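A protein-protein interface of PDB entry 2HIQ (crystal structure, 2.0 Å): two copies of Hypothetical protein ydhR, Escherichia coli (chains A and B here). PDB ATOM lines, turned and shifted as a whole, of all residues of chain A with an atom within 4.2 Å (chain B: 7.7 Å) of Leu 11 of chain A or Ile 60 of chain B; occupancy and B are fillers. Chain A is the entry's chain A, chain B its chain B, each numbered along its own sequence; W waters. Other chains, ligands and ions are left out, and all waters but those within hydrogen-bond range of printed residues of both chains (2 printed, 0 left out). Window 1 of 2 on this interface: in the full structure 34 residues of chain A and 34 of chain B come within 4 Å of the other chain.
CD1 of Leu 11 of chain A touches CG1 of Val 47 of chain B, 3.6 Å away.
CD1 of Leu 11 of chain A touches CG2 of Thr 49 of chain B, 3.8 Å away.
CG1 of Ile 60 of chain B touches CD1 of Leu 11 of chain A, 3.6 Å away.
Gln 13 of chain A touches Ile 60 of chain B.
Ile 60 of chain B touches Ile 60 of chain A.
Lys 91 of chain A touches His 15 of chain B.
Phe 93 of chain A touches His 15 of chain B (CZ to CB, 3.6 Å).
Thr 49 of chain B touches Phe 93 of chain A.
Phe 93 of chain A touches Glu 50 of chain B (C to O, 3.8 Å).
CA of Val 95 of chain A touches O of Trp 48 of chain B, at 3.4 Å.
Hydrophobic or aromatic side chains of chain A that line the printed part of chain B: Leu 11, Ile 60, Phe 93 and Val 95.
Printed residues of chain B that touch a printed residue of chain A: Leu 11, Gln 13, His 15, Val 47, Trp 48, Thr 49, Glu 50 and Ile 60.
N of Leu 11 of chain A is in hydrogen-bond range of O of Phe 93 of chain A (2.8 Å).
O of Thr 49 of chain B lies within hydrogen-bond range of N of Gly 58 of chain B (3.0 Å).
The backbone NH of Lys 91 of chain A lies within hydrogen-bond range of the backbone carbonyl oxygen of Gln 13 of chain A, at 3.0 Å.
The backbone carbonyl oxygen (O) of Ile 60 of chain B sits at hydrogen-bond distance from the backbone NH (N) of Val 47 of chain B, at 2.8 Å.
OG1 of Thr 49 of chain B sits at hydrogen-bond distance from N of Gly 59 of chain B (3.3 Å).
Leu 11 of chain A touches three residues of chain B.
Of the printed residues of chain B, Gln 13 of chain A touches Gln 13, His 15 and Ile 60.
Printed residues of chain A within 4 Å of Trp 48 of chain B: Val 95 (3.4 Å).
Of the printed residues of chain B, Val 95 of chain A touches Val 47 and Trp 48.
Printed residues of chain A within 4 Å of Val 47 of chain B: Leu 11 and Val 95.
Of the printed residues of chain B, Ile 60 of chain A touches Leu 11, Gln 13 and Ile 60.
The nearest printed residue of chain A that does not touch Ile 60 of chain B is Phe 93 of chain A (6.5 Å).
The nearest printed residue of chain B that does not touch Lys 91 of chain A is Gln 13 of chain B (6.8 Å).
Water W2 lies within hydrogen-bond range of the side-chain amide oxygen (OE1) of Gln 13 of chain A, the backbone carbonyl oxygen (O) of Leu 14 of chain B and the side-chain hydroxyl (OG1) of Thr 49 of chain B.
Water W1 lies within hydrogen-bond range of the backbone carbonyl oxygen of Gln 13 of chain A (3.3 Å) and the side-chain amide nitrogen of Gln 13 of chain B (3.4 Å).
Leu 11 of chain A touches Ile 60 of chain B, and with the chains exchanged Ile 60 of chain A touches Leu 11 of chain B.
Gln 13 of chain A touches its own counterpart, Gln 13 of chain B.
Gln 13 of chain A touches Ile 60 of chain B, and with the chains exchanged Ile 60 of chain A touches Gln 13 of chain B.
Ile 60 of chain B touches its own counterpart, Ile 60 of chain A.
Of the 15 pairs that touch across the chains among the printed residues, 6 have their exchanged pair printed and touching as well.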
ATOM      1  N   THR A  10       0.943 -13.485   0.026  1.00  0.00           N
ATOM      2  CA  THR A  10       0.624 -12.749  -1.187  1.00  0.00           C
ATOM      3  C   THR A  10       1.875 -12.163  -1.807  1.00  0.00           C
ATOM      4  O   THR A  10       2.709 -11.600  -1.105  1.00  0.00           O
ATOM      5  CB  THR A  10      -0.366 -11.611  -0.895  1.00  0.00           C
ATOM      6  OG1 THR A  10      -1.626 -12.164  -0.500  1.00  0.00           O
ATOM      7  CG2 THR A  10      -0.566 -10.740  -2.135  1.00  0.00           C
ATOM      8  N   LEU A  11       2.007 -12.299  -3.121  1.00  0.00           N
ATOM      9  CA  LEU A  11       3.170 -11.761  -3.799  1.00  0.00           C
ATOM     10  C   LEU A  11       2.750 -10.565  -4.628  1.00  0.00           C
ATOM     11  O   LEU A  11       1.762 -10.612  -5.363  1.00  0.00           O
ATOM     12  CB  LEU A  11       3.825 -12.819  -4.697  1.00  0.00           C
ATOM     13  CG  LEU A  11       5.124 -12.366  -5.381  1.00  0.00           C
ATOM     14  CD1 LEU A  11       6.006 -13.558  -5.653  1.00  0.00           C
ATOM     15  CD2 LEU A  11       4.799 -11.620  -6.667  1.00  0.00           C
ATOM     16  N   LEU A  12       3.493  -9.475  -4.482  1.00  0.00           N
ATOM     17  CA  LEU A  12       3.216  -8.269  -5.238  1.00  0.00           C
ATOM     18  C   LEU A  12       4.356  -8.085  -6.234  1.00  0.00           C
ATOM     19  O   LEU A  12       5.519  -8.088  -5.852  1.00  0.00           O
ATOM     20  CB  LEU A  12       3.151  -7.067  -4.288  1.00  0.00           C
ATOM     21  CG  LEU A  12       3.025  -5.667  -4.892  1.00  0.00           C
ATOM     22  CD1 LEU A  12       1.721  -5.547  -5.678  1.00  0.00           C
ATOM     23  CD2 LEU A  12       3.051  -4.628  -3.761  1.00  0.00           C
ATOM     24  N   GLN A  13       4.032  -7.967  -7.513  1.00  0.00           N
ATOM     25  CA  GLN A  13       5.070  -7.728  -8.500  1.00  0.00           C
ATOM     26  C   GLN A  13       4.751  -6.390  -9.143  1.00  0.00           C
ATOM     27  O   GLN A  13       3.618  -6.145  -9.566  1.00  0.00           O
ATOM     28  CB  GLN A  13       5.139  -8.840  -9.550  1.00  0.00           C
ATOM     29  CG  GLN A  13       3.883  -9.082 -10.355  1.00  0.00           C
ATOM     30  CD  GLN A  13       4.062 -10.257 -11.311  1.00  0.00           C
ATOM     31  OE1 GLN A  13       4.493 -11.340 -10.904  1.00  0.00           O
ATOM     32  NE2 GLN A  13       3.734 -10.048 -12.577  1.00  0.00           N
ATOM     33  N   ILE A  60       9.681  -7.167  -6.384  1.00  0.00           N
ATOM     34  CA  ILE A  60       8.829  -8.313  -6.108  1.00  0.00           C
ATOM     35  C   ILE A  60       8.725  -8.280  -4.592  1.00  0.00           C
ATOM     36  O   ILE A  60       9.744  -8.295  -3.902  1.00  0.00           O
ATOM     37  CB  ILE A  60       9.490  -9.648  -6.528  1.00  0.00           C
ATOM     38  CG1 ILE A  60       9.801  -9.633  -8.022  1.00  0.00           C
ATOM     39  CG2 ILE A  60       8.578 -10.821  -6.151  1.00  0.00           C
ATOM     40  CD1 ILE A  60       8.614  -9.332  -8.902  1.00  0.00           C
ATOM     41  N   TYR A  61       7.503  -8.226  -4.079  1.00  0.00           N
ATOM     42  CA  TYR A  61       7.280  -8.155  -2.644  1.00  0.00           C
ATOM     43  C   TYR A  61       6.481  -9.342  -2.122  1.00  0.00           C
ATOM     44  O   TYR A  61       5.535  -9.784  -2.772  1.00  0.00           O
ATOM     45  CB  TYR A  61       6.451  -6.918  -2.282  1.00  0.00           C
ATOM     46  CG  TYR A  61       7.028  -5.546  -2.556  1.00  0.00           C
ATOM     47  CD1 TYR A  61       7.367  -4.696  -1.500  1.00  0.00           C
ATOM     48  CD2 TYR A  61       7.116  -5.047  -3.860  1.00  0.00           C
ATOM     49  CE1 TYR A  61       7.771  -3.378  -1.726  1.00  0.00           C
ATOM     50  CE2 TYR A  61       7.524  -3.732  -4.103  1.00  0.00           C
ATOM     51  CZ  TYR A  61       7.846  -2.901  -3.024  1.00  0.00           C
ATOM     52  OH  TYR A  61       8.243  -1.599  -3.260  1.00  0.00           O
ATOM     53  N   LYS A  91       0.763  -6.598 -10.328  1.00  0.00           N
ATOM     54  CA  LYS A  91      -0.131  -7.734 -10.200  1.00  0.00           C
ATOM     55  C   LYS A  91      -0.015  -8.269  -8.787  1.00  0.00           C
ATOM     56  O   LYS A  91       1.057  -8.235  -8.180  1.00  0.00           O
ATOM     57  CB  LYS A  91       0.215  -8.824 -11.219  1.00  0.00           C
ATOM     58  CG  LYS A  91       0.151  -8.328 -12.651  1.00  0.00           C
ATOM     59  CD  LYS A  91      -0.146  -9.446 -13.628  1.00  0.00           C
ATOM     60  CE  LYS A  91      -1.576  -9.945 -13.497  1.00  0.00           C
ATOM     61  NZ  LYS A  91      -2.577  -9.021 -14.094  1.00  0.00           N
ATOM     62  N   VAL A  92      -1.141  -8.730  -8.259  1.00  0.00           N
ATOM     63  CA  VAL A  92      -1.196  -9.288  -6.920  1.00  0.00           C
ATOM     64  C   VAL A  92      -1.546 -10.760  -7.108  1.00  0.00           C
ATOM     65  O   VAL A  92      -2.503 -11.090  -7.814  1.00  0.00           O
ATOM     66  CB  VAL A  92      -2.287  -8.594  -6.079  1.00  0.00           C
ATOM     67  CG1 VAL A  92      -2.265  -9.117  -4.658  1.00  0.00           C
ATOM     68  CG2 VAL A  92      -2.074  -7.092  -6.101  1.00  0.00           C
ATOM     69  N   PHE A  93      -0.760 -11.636  -6.494  1.00  0.00           N
ATOM     70  CA  PHE A  93      -0.964 -13.078  -6.611  1.00  0.00           C
ATOM     71  C   PHE A  93      -0.887 -13.803  -5.277  1.00  0.00           C
ATOM     72  O   PHE A  93      -0.312 -13.305  -4.310  1.00  0.00           O
ATOM     73  CB  PHE A  93       0.118 -13.703  -7.500  1.00  0.00           C
ATOM     74  CG  PHE A  93       0.040 -13.315  -8.949  1.00  0.00           C
ATOM     75  CD1 PHE A  93      -1.052 -13.683  -9.730  1.00  0.00           C
ATOM     76  CD2 PHE A  93       1.090 -12.630  -9.550  1.00  0.00           C
ATOM     77  CE1 PHE A  93      -1.090 -13.376 -11.090  1.00  0.00           C
ATOM     78  CE2 PHE A  93       1.059 -12.321 -10.905  1.00  0.00           C
ATOM     79  CZ  PHE A  93      -0.033 -12.695 -11.678  1.00  0.00           C
ATOM     80  N   VAL A  95       0.567 -17.061  -3.319  1.00  0.00           N
ATOM     81  CA  VAL A  95       1.750 -17.878  -3.514  1.00  0.00           C
ATOM     82  C   VAL A  95       1.374 -19.334  -3.258  1.00  0.00           C
ATOM     83  O   VAL A  95       0.638 -19.623  -2.315  1.00  0.00           O
ATOM     84  CB  VAL A  95       2.870 -17.496  -2.523  1.00  0.00           C
ATOM     85  CG1 VAL A  95       3.999 -18.523  -2.590  1.00  0.00           C
ATOM     86  CG2 VAL A  95       3.416 -16.105  -2.853  1.00  0.00           C
ATOM     87  N   LEU B  11      16.593 -11.872 -12.608  1.00  0.00           N
ATOM     88  CA  LEU B  11      15.265 -12.248 -12.159  1.00  0.00           C
ATOM     89  C   LEU B  11      14.310 -12.331 -13.333  1.00  0.00           C
ATOM     90  O   LEU B  11      14.297 -11.476 -14.220  1.00  0.00           O
ATOM     91  CB  LEU B  11      14.737 -11.241 -11.131  1.00  0.00           C
ATOM     92  CG  LEU B  11      13.385 -11.565 -10.475  1.00  0.00           C
ATOM     93  CD1 LEU B  11      13.343 -10.956  -9.090  1.00  0.00           C
ATOM     94  CD2 LEU B  11      12.240 -11.054 -11.329  1.00  0.00           C
ATOM     95  N   LEU B  12      13.503 -13.379 -13.329  1.00  0.00           N
ATOM     96  CA  LEU B  12      12.539 -13.579 -14.382  1.00  0.00           C
ATOM     97  C   LEU B  12      11.161 -13.490 -13.742  1.00  0.00           C
ATOM     98  O   LEU B  12      10.891 -14.172 -12.753  1.00  0.00           O
ATOM     99  CB  LEU B  12      12.756 -14.964 -14.996  1.00  0.00           C
ATOM    100  CG  LEU B  12      11.901 -15.443 -16.161  1.00  0.00           C
ATOM    101  CD1 LEU B  12      12.114 -14.539 -17.384  1.00  0.00           C
ATOM    102  CD2 LEU B  12      12.310 -16.879 -16.504  1.00  0.00           C
ATOM    103  N   GLN B  13      10.307 -12.612 -14.254  1.00  0.00           N
ATOM    104  CA  GLN B  13       8.962 -12.554 -13.714  1.00  0.00           C
ATOM    105  C   GLN B  13       8.023 -12.916 -14.845  1.00  0.00           C
ATOM    106  O   GLN B  13       8.073 -12.339 -15.931  1.00  0.00           O
ATOM    107  CB  GLN B  13       8.618 -11.186 -13.090  1.00  0.00           C
ATOM    108  CG  GLN B  13       8.515  -9.988 -14.007  1.00  0.00           C
ATOM    109  CD  GLN B  13       7.960  -8.762 -13.267  1.00  0.00           C
ATOM    110  OE1 GLN B  13       8.537  -8.305 -12.277  1.00  0.00           O
ATOM    111  NE2 GLN B  13       6.840  -8.235 -13.748  1.00  0.00           N
ATOM    112  N   LEU B  14       7.190 -13.918 -14.581  1.00  0.00           N
ATOM    113  CA  LEU B  14       6.244 -14.428 -15.567  1.00  0.00           C
ATOM    114  C   LEU B  14       4.857 -14.668 -15.015  1.00  0.00           C
ATOM    115  O   LEU B  14       4.702 -15.038 -13.857  1.00  0.00           O
ATOM    116  CB  LEU B  14       6.732 -15.768 -16.115  1.00  0.00           C
ATOM    117  CG  LEU B  14       7.640 -15.845 -17.332  1.00  0.00           C
ATOM    118  CD1 LEU B  14       8.888 -15.040 -17.098  1.00  0.00           C
ATOM    119  CD2 LEU B  14       7.985 -17.313 -17.595  1.00  0.00           C
ATOM    120  N   HIS B  15       3.851 -14.453 -15.854  1.00  0.00           N
ATOM    121  CA  HIS B  15       2.473 -14.738 -15.490  1.00  0.00           C
ATOM    122  C   HIS B  15       1.716 -14.932 -16.800  1.00  0.00           C
ATOM    123  O   HIS B  15       2.217 -14.592 -17.878  1.00  0.00           O
ATOM    124  CB  HIS B  15       1.855 -13.631 -14.613  1.00  0.00           C
ATOM    125  CG  HIS B  15       1.536 -12.362 -15.338  1.00  0.00           C
ATOM    126  ND1 HIS B  15       0.349 -12.171 -16.014  1.00  0.00           N
ATOM    127  CD2 HIS B  15       2.224 -11.204 -15.454  1.00  0.00           C
ATOM    128  CE1 HIS B  15       0.322 -10.948 -16.513  1.00  0.00           C
ATOM    129  NE2 HIS B  15       1.448 -10.340 -16.187  1.00  0.00           N
ATOM    130  N   PHE B  43      19.641 -22.224 -12.294  1.00  0.00           N
ATOM    131  CA  PHE B  43      18.468 -22.005 -11.461  1.00  0.00           C
ATOM    132  C   PHE B  43      18.818 -21.854  -9.987  1.00  0.00           C
ATOM    133  O   PHE B  43      19.620 -22.615  -9.453  1.00  0.00           O
ATOM    134  CB  PHE B  43      17.488 -23.163 -11.628  1.00  0.00           C
ATOM    135  CG  PHE B  43      16.253 -23.022 -10.795  1.00  0.00           C
ATOM    136  CD1 PHE B  43      15.260 -22.119 -11.154  1.00  0.00           C
ATOM    137  CD2 PHE B  43      16.086 -23.784  -9.645  1.00  0.00           C
ATOM    138  CE1 PHE B  43      14.117 -21.976 -10.379  1.00  0.00           C
ATOM    139  CE2 PHE B  43      14.947 -23.650  -8.861  1.00  0.00           C
ATOM    140  CZ  PHE B  43      13.958 -22.745  -9.229  1.00  0.00           C
ATOM    141  N   TRP B  45      16.078 -20.258  -7.482  1.00  0.00           N
ATOM    142  CA  TRP B  45      14.820 -20.470  -6.790  1.00  0.00           C
ATOM    143  C   TRP B  45      13.645 -19.949  -7.597  1.00  0.00           C
ATOM    144  O   TRP B  45      13.810 -19.201  -8.562  1.00  0.00           O
ATOM    145  CB  TRP B  45      14.820 -19.843  -5.380  1.00  0.00           C
ATOM    146  CG  TRP B  45      15.159 -18.383  -5.306  1.00  0.00           C
ATOM    147  CD1 TRP B  45      16.367 -17.831  -4.973  1.00  0.00           C
ATOM    148  CD2 TRP B  45      14.280 -17.286  -5.579  1.00  0.00           C
ATOM    149  NE1 TRP B  45      16.292 -16.458  -5.022  1.00  0.00           N
ATOM    150  CE2 TRP B  45      15.023 -16.096  -5.393  1.00  0.00           C
ATOM    151  CE3 TRP B  45      12.937 -17.192  -5.967  1.00  0.00           C
ATOM    152  CZ2 TRP B  45      14.464 -14.828  -5.581  1.00  0.00           C
ATOM    153  CZ3 TRP B  45      12.380 -15.932  -6.154  1.00  0.00           C
ATOM    154  CH2 TRP B  45      13.145 -14.765  -5.962  1.00  0.00           C
ATOM    155  N   LYS B  46      12.452 -20.384  -7.212  1.00  0.00           N
ATOM    156  CA  LYS B  46      11.238 -19.973  -7.887  1.00  0.00           C
ATOM    157  C   LYS B  46      10.102 -19.851  -6.904  1.00  0.00           C
ATOM    158  O   LYS B  46       9.958 -20.672  -5.998  1.00  0.00           O
ATOM    159  CB  LYS B  46      10.825 -20.985  -8.963  1.00  0.00           C
ATOM    160  CG  LYS B  46       9.428 -20.700  -9.534  1.00  0.00           C
ATOM    161  CD  LYS B  46       8.944 -21.771 -10.513  1.00  0.00           C
ATOM    162  CE  LYS B  46       7.579 -21.403 -11.080  1.00  0.00           C
ATOM    163  NZ  LYS B  46       6.994 -22.452 -11.964  1.00  0.00           N
ATOM    164  N   VAL B  47       9.300 -18.812  -7.086  1.00  0.00           N
ATOM    165  CA  VAL B  47       8.132 -18.611  -6.254  1.00  0.00           C
ATOM    166  C   VAL B  47       6.970 -18.792  -7.217  1.00  0.00           C
ATOM    167  O   VAL B  47       6.889 -18.104  -8.233  1.00  0.00           O
ATOM    168  CB  VAL B  47       8.086 -17.194  -5.643  1.00  0.00           C
ATOM    169  CG1 VAL B  47       6.778 -17.005  -4.890  1.00  0.00           C
ATOM    170  CG2 VAL B  47       9.266 -16.993  -4.695  1.00  0.00           C
ATOM    171  N   TRP B  48       6.100 -19.752  -6.917  1.00  0.00           N
ATOM    172  CA  TRP B  48       4.945 -20.018  -7.760  1.00  0.00           C
ATOM    173  C   TRP B  48       3.830 -19.064  -7.382  1.00  0.00           C
ATOM    174  O   TRP B  48       3.500 -18.921  -6.208  1.00  0.00           O
ATOM    175  CB  TRP B  48       4.452 -21.460  -7.588  1.00  0.00           C
ATOM    176  CG  TRP B  48       5.420 -22.506  -8.065  1.00  0.00           C
ATOM    177  CD1 TRP B  48       6.636 -22.810  -7.520  1.00  0.00           C
ATOM    178  CD2 TRP B  48       5.260 -23.374  -9.194  1.00  0.00           C
ATOM    179  NE1 TRP B  48       7.242 -23.812  -8.237  1.00  0.00           N
ATOM    180  CE2 TRP B  48       6.418 -24.179  -9.270  1.00  0.00           C
ATOM    181  CE3 TRP B  48       4.251 -23.550 -10.150  1.00  0.00           C
ATOM    182  CZ2 TRP B  48       6.594 -25.151 -10.266  1.00  0.00           C
ATOM    183  CZ3 TRP B  48       4.427 -24.515 -11.140  1.00  0.00           C
ATOM    184  CH2 TRP B  48       5.588 -25.301 -11.187  1.00  0.00           C
ATOM    185  N   THR B  49       3.252 -18.414  -8.378  1.00  0.00           N
ATOM    186  CA  THR B  49       2.177 -17.468  -8.139  1.00  0.00           C
ATOM    187  C   THR B  49       0.908 -17.973  -8.799  1.00  0.00           C
ATOM    188  O   THR B  49       0.961 -18.677  -9.810  1.00  0.00           O
ATOM    189  CB  THR B  49       2.526 -16.096  -8.729  1.00  0.00           C
ATOM    190  OG1 THR B  49       2.825 -16.254 -10.121  1.00  0.00           O
ATOM    191  CG2 THR B  49       3.727 -15.506  -8.023  1.00  0.00           C
ATOM    192  N   GLU B  50      -0.233 -17.610  -8.230  1.00  0.00           N
ATOM    193  CA  GLU B  50      -1.506 -18.040  -8.784  1.00  0.00           C
ATOM    194  C   GLU B  50      -2.631 -17.144  -8.313  1.00  0.00           C
ATOM    195  O   GLU B  50      -2.580 -16.598  -7.216  1.00  0.00           O
ATOM    196  CB  GLU B  50      -1.813 -19.480  -8.361  1.00  0.00           C
ATOM    197  CG  GLU B  50      -1.873 -19.672  -6.854  1.00  0.00           C
ATOM    198  CD  GLU B  50      -2.498 -20.998  -6.440  1.00  0.00           C
ATOM    199  OE1 GLU B  50      -3.690 -21.215  -6.741  1.00  0.00           O
ATOM    200  OE2 GLU B  50      -1.798 -21.813  -5.807  1.00  0.00           O
ATOM    201  N   GLY B  58       1.706 -18.042 -12.649  1.00  0.00           N
ATOM    202  CA  GLY B  58       3.025 -17.697 -13.141  1.00  0.00           C
ATOM    203  C   GLY B  58       4.079 -18.021 -12.111  1.00  0.00           C
ATOM    204  O   GLY B  58       3.906 -18.913 -11.275  1.00  0.00           O
ATOM    205  N   GLY B  59       5.184 -17.294 -12.166  1.00  0.00           N
ATOM    206  CA  GLY B  59       6.241 -17.535 -11.212  1.00  0.00           C
ATOM    207  C   GLY B  59       7.321 -16.484 -11.286  1.00  0.00           C
ATOM    208  O   GLY B  59       7.443 -15.772 -12.282  1.00  0.00           O
ATOM    209  N   ILE B  60       8.083 -16.381 -10.204  1.00  0.00           N
ATOM    210  CA  ILE B  60       9.192 -15.454 -10.116  1.00  0.00           C
ATOM    211  C   ILE B  60      10.405 -16.354 -10.009  1.00  0.00           C
ATOM    212  O   ILE B  60      10.456 -17.221  -9.139  1.00  0.00           O
ATOM    213  CB  ILE B  60       9.127 -14.586  -8.842  1.00  0.00           C
ATOM    214  CG1 ILE B  60       7.801 -13.829  -8.789  1.00  0.00           C
ATOM    215  CG2 ILE B  60      10.324 -13.638  -8.810  1.00  0.00           C
ATOM    216  CD1 ILE B  60       7.559 -12.920  -9.969  1.00  0.00           C
ATOM    217  N   TYR B  61      11.368 -16.164 -10.902  1.00  0.00           N
ATOM    218  CA  TYR B  61      12.572 -16.972 -10.896  1.00  0.00           C
ATOM    219  C   TYR B  61      13.825 -16.155 -10.679  1.00  0.00           C
ATOM    220  O   TYR B  61      13.906 -14.985 -11.060  1.00  0.00           O
ATOM    221  CB  TYR B  61      12.761 -17.688 -12.232  1.00  0.00           C
ATOM    222  CG  TYR B  61      11.683 -18.650 -12.639  1.00  0.00           C
ATOM    223  CD1 TYR B  61      11.919 -20.027 -12.632  1.00  0.00           C
ATOM    224  CD2 TYR B  61      10.459 -18.190 -13.123  1.00  0.00           C
ATOM    225  CE1 TYR B  61      10.968 -20.916 -13.108  1.00  0.00           C
ATOM    226  CE2 TYR B  61       9.502 -19.076 -13.601  1.00  0.00           C
ATOM    227  CZ  TYR B  61       9.763 -20.433 -13.595  1.00  0.00           C
ATOM    228  OH  TYR B  61       8.823 -21.310 -14.098  1.00  0.00           O
ATOM    229  N   LEU B  62      14.818 -16.811 -10.100  1.00  0.00           N
ATOM    230  CA  LEU B  62      16.109 -16.197  -9.876  1.00  0.00           C
ATOM    231  C   LEU B  62      17.129 -17.131 -10.530  1.00  0.00           C
ATOM    232  O   LEU B  62      17.163 -18.322 -10.225  1.00  0.00           O
ATOM    233  CB  LEU B  62      16.383 -16.085  -8.379  1.00  0.00           C
ATOM    234  CG  LEU B  62      17.177 -14.854  -7.935  1.00  0.00           C
ATOM    235  CD1 LEU B  62      18.578 -14.900  -8.506  1.00  0.00           C
ATOM    236  CD2 LEU B  62      16.453 -13.597  -8.402  1.00  0.00           C
ATOM    237  N   PHE B  63      17.930 -16.599 -11.447  1.00  0.00           N
ATOM    238  CA  PHE B  63      18.963 -17.378 -12.127  1.00  0.00           C
ATOM    239  C   PHE B  63      20.325 -16.729 -11.889  1.00  0.00           C
ATOM    240  O   PHE B  63      20.412 -15.531 -11.613  1.00  0.00           O
ATOM    241  CB  PHE B  63      18.695 -17.442 -13.630  1.00  0.00           C
ATOM    242  CG  PHE B  63      17.607 -18.400 -14.011  1.00  0.00           C
ATOM    243  CD1 PHE B  63      17.883 -19.746 -14.226  1.00  0.00           C
ATOM    244  CD2 PHE B  63      16.297 -17.959 -14.128  1.00  0.00           C
ATOM    245  CE1 PHE B  63      16.860 -20.642 -14.556  1.00  0.00           C
ATOM    246  CE2 PHE B  63      15.271 -18.842 -14.456  1.00  0.00           C
ATOM    247  CZ  PHE B  63      15.552 -20.185 -14.669  1.00  0.00           C
HETATM  248  O   HOH W   1       4.640  -5.847 -12.699  1.00  0.00           O
HETATM  249  O   HOH W   2       4.104 -14.024 -11.329  1.00  0.00           O
